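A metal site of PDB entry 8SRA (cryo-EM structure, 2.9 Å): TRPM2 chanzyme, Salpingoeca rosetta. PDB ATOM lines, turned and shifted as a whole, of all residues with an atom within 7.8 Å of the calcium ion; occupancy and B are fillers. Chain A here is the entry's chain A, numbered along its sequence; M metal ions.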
ATOM      1  N   LEU A 846      34.510 -13.338   0.472  1.00  0.00           N
ATOM      2  CA  LEU A 846      33.305 -13.794  -0.228  1.00  0.00           C
ATOM      3  C   LEU A 846      32.292 -12.669  -0.398  1.00  0.00           C
ATOM      4  O   LEU A 846      31.615 -12.601  -1.431  1.00  0.00           O
ATOM      5  CB  LEU A 846      32.643 -14.965   0.466  1.00  0.00           C
ATOM      6  CG  LEU A 846      33.264 -16.341   0.381  1.00  0.00           C
ATOM      7  CD1 LEU A 846      32.362 -17.271   1.109  1.00  0.00           C
ATOM      8  CD2 LEU A 846      33.407 -16.752  -1.043  1.00  0.00           C
ATOM      9  N   GLU A 849      33.549 -10.309  -3.032  1.00  0.00           N
ATOM     10  CA  GLU A 849      33.321 -10.938  -4.332  1.00  0.00           C
ATOM     11  C   GLU A 849      31.861 -10.819  -4.774  1.00  0.00           C
ATOM     12  O   GLU A 849      31.587 -10.606  -5.967  1.00  0.00           O
ATOM     13  CB  GLU A 849      33.799 -12.394  -4.292  1.00  0.00           C
ATOM     14  CG  GLU A 849      33.501 -13.305  -5.507  1.00  0.00           C
ATOM     15  CD  GLU A 849      34.072 -12.854  -6.861  1.00  0.00           C
ATOM     16  OE1 GLU A 849      35.085 -12.130  -6.941  1.00  0.00           O
ATOM     17  OE2 GLU A 849      33.466 -13.239  -7.878  1.00  0.00           O
ATOM     18  N   GLU A 850      30.911 -10.972  -3.825  1.00  0.00           N
ATOM     19  CA  GLU A 850      29.474 -10.771  -4.085  1.00  0.00           C
ATOM     20  C   GLU A 850      29.156  -9.315  -4.460  1.00  0.00           C
ATOM     21  O   GLU A 850      28.280  -9.070  -5.301  1.00  0.00           O
ATOM     22  CB  GLU A 850      28.614 -11.234  -2.919  1.00  0.00           C
ATOM     23  CG  GLU A 850      28.527 -12.745  -2.780  1.00  0.00           C
ATOM     24  CD  GLU A 850      28.275 -13.450  -4.097  1.00  0.00           C
ATOM     25  OE1 GLU A 850      27.170 -13.321  -4.649  1.00  0.00           O
ATOM     26  OE2 GLU A 850      29.182 -14.161  -4.577  1.00  0.00           O
ATOM     27  N   LEU A 851      29.802  -8.343  -3.766  1.00  0.00           N
ATOM     28  CA  LEU A 851      29.667  -6.914  -4.114  1.00  0.00           C
ATOM     29  C   LEU A 851      30.228  -6.609  -5.498  1.00  0.00           C
ATOM     30  O   LEU A 851      29.680  -5.740  -6.193  1.00  0.00           O
ATOM     31  CB  LEU A 851      30.310  -5.999  -3.070  1.00  0.00           C
ATOM     32  CG  LEU A 851      29.706  -5.948  -1.670  1.00  0.00           C
ATOM     33  CD1 LEU A 851      30.452  -4.944  -0.814  1.00  0.00           C
ATOM     34  CD2 LEU A 851      28.238  -5.610  -1.731  1.00  0.00           C
ATOM     35  N   GLN A 853      30.437  -8.789  -7.972  1.00  0.00           N
ATOM     36  CA  GLN A 853      29.425  -9.385  -8.858  1.00  0.00           C
ATOM     37  C   GLN A 853      28.197  -8.498  -8.995  1.00  0.00           C
ATOM     38  O   GLN A 853      27.527  -8.550 -10.035  1.00  0.00           O
ATOM     39  CB  GLN A 853      29.020 -10.779  -8.393  1.00  0.00           C
ATOM     40  CG  GLN A 853      30.039 -11.839  -8.736  1.00  0.00           C
ATOM     41  CD  GLN A 853      29.793 -13.129  -8.007  1.00  0.00           C
ATOM     42  OE1 GLN A 853      28.690 -13.413  -7.542  1.00  0.00           O
ATOM     43  NE2 GLN A 853      30.838 -13.947  -7.890  1.00  0.00           N
ATOM     44  N   MET A 854      27.782  -7.837  -7.899  1.00  0.00           N
ATOM     45  CA  MET A 854      26.676  -6.872  -7.943  1.00  0.00           C
ATOM     46  C   MET A 854      26.971  -5.678  -8.858  1.00  0.00           C
ATOM     47  O   MET A 854      26.074  -5.210  -9.561  1.00  0.00           O
ATOM     48  CB  MET A 854      26.377  -6.333  -6.546  1.00  0.00           C
ATOM     49  CG  MET A 854      25.240  -6.943  -5.835  1.00  0.00           C
ATOM     50  SD  MET A 854      24.971  -6.147  -4.242  1.00  0.00           S
ATOM     51  CE  MET A 854      23.763  -7.237  -3.505  1.00  0.00           C
ATOM     52  N   TYR A 863      21.237 -10.089 -11.008  1.00  0.00           N
ATOM     53  CA  TYR A 863      22.058 -10.756 -10.002  1.00  0.00           C
ATOM     54  C   TYR A 863      21.184 -11.523  -9.010  1.00  0.00           C
ATOM     55  O   TYR A 863      21.430 -12.696  -8.716  1.00  0.00           O
ATOM     56  CB  TYR A 863      22.918  -9.714  -9.274  1.00  0.00           C
ATOM     57  CG  TYR A 863      23.642 -10.192  -8.021  1.00  0.00           C
ATOM     58  CD1 TYR A 863      24.838 -10.899  -8.150  1.00  0.00           C
ATOM     59  CD2 TYR A 863      23.163  -9.858  -6.724  1.00  0.00           C
ATOM     60  CE1 TYR A 863      25.543 -11.332  -7.010  1.00  0.00           C
ATOM     61  CE2 TYR A 863      23.838 -10.318  -5.593  1.00  0.00           C
ATOM     62  CZ  TYR A 863      25.022 -11.028  -5.751  1.00  0.00           C
ATOM     63  OH  TYR A 863      25.699 -11.449  -4.646  1.00  0.00           O
ATOM     64  N   ASP A 866      19.207 -15.074  -9.853  1.00  0.00           N
ATOM     65  CA  ASP A 866      19.943 -16.332  -9.716  1.00  0.00           C
ATOM     66  C   ASP A 866      19.816 -16.858  -8.284  1.00  0.00           C
ATOM     67  O   ASP A 866      19.991 -16.100  -7.336  1.00  0.00           O
ATOM     68  CB  ASP A 866      21.407 -16.126 -10.079  1.00  0.00           C
ATOM     69  CG  ASP A 866      22.150 -17.415 -10.286  1.00  0.00           C
ATOM     70  OD1 ASP A 866      21.491 -18.447 -10.545  1.00  0.00           O
ATOM     71  OD2 ASP A 866      23.390 -17.409 -10.209  1.00  0.00           O
ATOM     72  N   TRP A 868      21.792 -19.149  -6.712  1.00  0.00           N
ATOM     73  CA  TRP A 868      23.093 -19.330  -6.067  1.00  0.00           C
ATOM     74  C   TRP A 868      23.606 -18.055  -5.431  1.00  0.00           C
ATOM     75  O   TRP A 868      24.284 -18.111  -4.387  1.00  0.00           O
ATOM     76  CB  TRP A 868      24.069 -19.871  -7.109  1.00  0.00           C
ATOM     77  CG  TRP A 868      23.554 -21.102  -7.800  1.00  0.00           C
ATOM     78  CD1 TRP A 868      23.231 -21.185  -9.119  1.00  0.00           C
ATOM     79  CD2 TRP A 868      23.320 -22.411  -7.249  1.00  0.00           C
ATOM     80  NE1 TRP A 868      22.802 -22.449  -9.430  1.00  0.00           N
ATOM     81  CE2 TRP A 868      22.847 -23.227  -8.308  1.00  0.00           C
ATOM     82  CE3 TRP A 868      23.467 -22.989  -5.983  1.00  0.00           C
ATOM     83  CZ2 TRP A 868      22.507 -24.567  -8.133  1.00  0.00           C
ATOM     84  CZ3 TRP A 868      23.122 -24.323  -5.796  1.00  0.00           C
ATOM     85  CH2 TRP A 868      22.653 -25.088  -6.870  1.00  0.00           C
ATOM     86  N   ASN A 869      23.285 -16.902  -6.043  1.00  0.00           N
ATOM     87  CA  ASN A 869      23.572 -15.601  -5.467  1.00  0.00           C
ATOM     88  C   ASN A 869      22.775 -15.345  -4.189  1.00  0.00           C
ATOM     89  O   ASN A 869      23.325 -14.779  -3.240  1.00  0.00           O
ATOM     90  CB  ASN A 869      23.295 -14.531  -6.507  1.00  0.00           C
ATOM     91  CG  ASN A 869      24.320 -14.556  -7.617  1.00  0.00           C
ATOM     92  OD1 ASN A 869      25.447 -14.987  -7.419  1.00  0.00           O
ATOM     93  ND2 ASN A 869      23.924 -14.094  -8.795  1.00  0.00           N
ATOM     94  N   ARG A 870      21.498 -15.793  -4.169  1.00  0.00           N
ATOM     95  CA  ARG A 870      20.637 -15.745  -2.981  1.00  0.00           C
ATOM     96  C   ARG A 870      21.187 -16.590  -1.842  1.00  0.00           C
ATOM     97  O   ARG A 870      21.151 -16.151  -0.678  1.00  0.00           O
ATOM     98  CB  ARG A 870      19.215 -16.170  -3.312  1.00  0.00           C
ATOM     99  CG  ARG A 870      18.577 -15.348  -4.377  1.00  0.00           C
ATOM    100  CD  ARG A 870      17.390 -16.045  -4.981  1.00  0.00           C
ATOM    101  NE  ARG A 870      16.360 -15.095  -5.389  1.00  0.00           N
ATOM    102  CZ  ARG A 870      15.106 -15.431  -5.653  1.00  0.00           C
ATOM    103  NH1 ARG A 870      14.694 -16.687  -5.567  1.00  0.00           N
ATOM    104  NH2 ARG A 870      14.255 -14.489  -6.021  1.00  0.00           N
ATOM    105  N   LEU A 871      21.699 -17.793  -2.182  1.00  0.00           N
ATOM    106  CA  LEU A 871      22.377 -18.686  -1.225  1.00  0.00           C
ATOM    107  C   LEU A 871      23.646 -18.058  -0.645  1.00  0.00           C
ATOM    108  O   LEU A 871      23.954 -18.290   0.529  1.00  0.00           O
ATOM    109  CB  LEU A 871      22.687 -20.035  -1.879  1.00  0.00           C
ATOM    110  CG  LEU A 871      21.511 -20.984  -2.008  1.00  0.00           C
ATOM    111  CD1 LEU A 871      21.954 -22.255  -2.673  1.00  0.00           C
ATOM    112  CD2 LEU A 871      20.907 -21.304  -0.670  1.00  0.00           C
ATOM    113  N   ASP A 872      24.394 -17.317  -1.487  1.00  0.00           N
ATOM    114  CA  ASP A 872      25.594 -16.581  -1.054  1.00  0.00           C
ATOM    115  C   ASP A 872      25.263 -15.497  -0.035  1.00  0.00           C
ATOM    116  O   ASP A 872      25.990 -15.348   0.969  1.00  0.00           O
ATOM    117  CB  ASP A 872      26.310 -15.988  -2.269  1.00  0.00           C
ATOM    118  CG  ASP A 872      27.233 -16.974  -2.924  1.00  0.00           C
ATOM    119  OD1 ASP A 872      27.870 -17.777  -2.204  1.00  0.00           O
ATOM    120  OD2 ASP A 872      27.324 -16.974  -4.168  1.00  0.00           O
ATOM    121  N   LEU A 873      24.161 -14.809  -0.242  1.00  0.00           N
ATOM    122  CA  LEU A 873      23.795 -13.734   0.700  1.00  0.00           C
ATOM    123  C   LEU A 873      23.339 -14.388   2.006  1.00  0.00           C
ATOM    124  O   LEU A 873      23.794 -13.949   3.066  1.00  0.00           O
ATOM    125  CB  LEU A 873      22.696 -12.878   0.055  1.00  0.00           C
ATOM    126  CG  LEU A 873      23.117 -12.118  -1.199  1.00  0.00           C
ATOM    127  CD1 LEU A 873      21.920 -11.418  -1.839  1.00  0.00           C
ATOM    128  CD2 LEU A 873      24.198 -11.110  -0.861  1.00  0.00           C
ATOM    129  N   ARG A 913      25.051 -25.056  -1.455  1.00  0.00           N
ATOM    130  CA  ARG A 913      25.629 -24.164  -2.492  1.00  0.00           C
ATOM    131  C   ARG A 913      26.713 -24.905  -3.242  1.00  0.00           C
ATOM    132  O   ARG A 913      27.001 -24.546  -4.367  1.00  0.00           O
ATOM    133  CB  ARG A 913      26.136 -22.884  -1.844  1.00  0.00           C
ATOM    134  CG  ARG A 913      27.116 -22.063  -2.672  1.00  0.00           C
ATOM    135  CD  ARG A 913      26.425 -21.259  -3.752  1.00  0.00           C
ATOM    136  NE  ARG A 913      27.314 -20.224  -4.258  1.00  0.00           N
ATOM    137  CZ  ARG A 913      28.360 -20.446  -5.041  1.00  0.00           C
ATOM    138  NH1 ARG A 913      28.656 -21.674  -5.429  1.00  0.00           N
ATOM    139  NH2 ARG A 913      29.101 -19.430  -5.443  1.00  0.00           N
ATOM    140  N   ARG A 916      26.158 -26.183  -6.975  1.00  0.00           N
ATOM    141  CA  ARG A 916      26.401 -25.298  -8.130  1.00  0.00           C
ATOM    142  C   ARG A 916      27.456 -25.860  -9.086  1.00  0.00           C
ATOM    143  O   ARG A 916      27.292 -25.801 -10.309  1.00  0.00           O
ATOM    144  CB  ARG A 916      26.805 -23.892  -7.662  1.00  0.00           C
ATOM    145  CG  ARG A 916      27.625 -22.969  -8.582  1.00  0.00           C
ATOM    146  CD  ARG A 916      26.732 -22.142  -9.501  1.00  0.00           C
ATOM    147  NE  ARG A 916      26.129 -22.887 -10.600  1.00  0.00           N
ATOM    148  CZ  ARG A 916      25.455 -22.339 -11.596  1.00  0.00           C
ATOM    149  NH1 ARG A 916      25.280 -21.032 -11.678  1.00  0.00           N
ATOM    150  NH2 ARG A 916      24.924 -23.122 -12.528  1.00  0.00           N
ATOM    151  N   GLU A1062      30.623 -16.775 -17.206  1.00  0.00           N
ATOM    152  CA  GLU A1062      30.791 -16.380 -15.806  1.00  0.00           C
ATOM    153  C   GLU A1062      32.211 -16.656 -15.308  1.00  0.00           C
ATOM    154  O   GLU A1062      32.794 -15.846 -14.576  1.00  0.00           O
ATOM    155  CB  GLU A1062      29.728 -17.088 -14.958  1.00  0.00           C
ATOM    156  CG  GLU A1062      29.868 -17.029 -13.447  1.00  0.00           C
ATOM    157  CD  GLU A1062      28.716 -17.681 -12.739  1.00  0.00           C
ATOM    158  OE1 GLU A1062      27.615 -17.741 -13.319  1.00  0.00           O
ATOM    159  OE2 GLU A1062      28.905 -18.150 -11.599  1.00  0.00           O
ATOM    160  N   ARG A1066      35.903 -14.010 -14.209  1.00  0.00           N
ATOM    161  CA  ARG A1066      36.187 -14.126 -12.788  1.00  0.00           C
ATOM    162  C   ARG A1066      37.706 -14.241 -12.591  1.00  0.00           C
ATOM    163  O   ARG A1066      38.376 -14.769 -13.487  1.00  0.00           O
ATOM    164  CB  ARG A1066      35.464 -15.368 -12.247  1.00  0.00           C
ATOM    165  CG  ARG A1066      35.772 -15.806 -10.825  1.00  0.00           C
ATOM    166  CD  ARG A1066      35.026 -16.986 -10.374  1.00  0.00           C
ATOM    167  NE  ARG A1066      35.114 -17.145  -8.927  1.00  0.00           N
ATOM    168  CZ  ARG A1066      34.214 -16.672  -8.072  1.00  0.00           C
ATOM    169  NH1 ARG A1066      33.155 -16.005  -8.494  1.00  0.00           N
ATOM    170  NH2 ARG A1066      34.398 -16.862  -6.778  1.00  0.00           N
HETATM  171 CA    CA M   1      27.761 -15.320  -6.303  1.00  0.00          CA
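The guanidinium group (NH1) of Arg 1066 lies close to the side-chain amide nitrogen (NE2) of Gln 853 (3.2 Å).
The side-chain amide nitrogen (NE2) of Gln 853 sits at hydrogen-bond distance from the side-chain carboxylate (OE2) of Glu 849 (2.7 Å).
The side-chain amide nitrogen (ND2) of Asn 869 lies within hydrogen-bond range of the backbone carbonyl oxygen (O) of Tyr 863, at 2.9 Å.
OD1 of Asp 872 lies within salt-bridge range of NE of Arg 913, at 3.2 Å.
The calcium ion is bound by the side-chain amide oxygen (OE1) of Gln 853 (2.5 Å).
The side-chain carboxylate (OE2) of Glu 850 binds the calcium ion (2.5 Å).
The side-chain amide oxygen (OD1) of Asn 869 binds the calcium ion (2.6 Å).
OE1 of Glu 850 binds the calcium ion (2.7 Å).
OD2 of Asp 872 is bound to the calcium ion.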
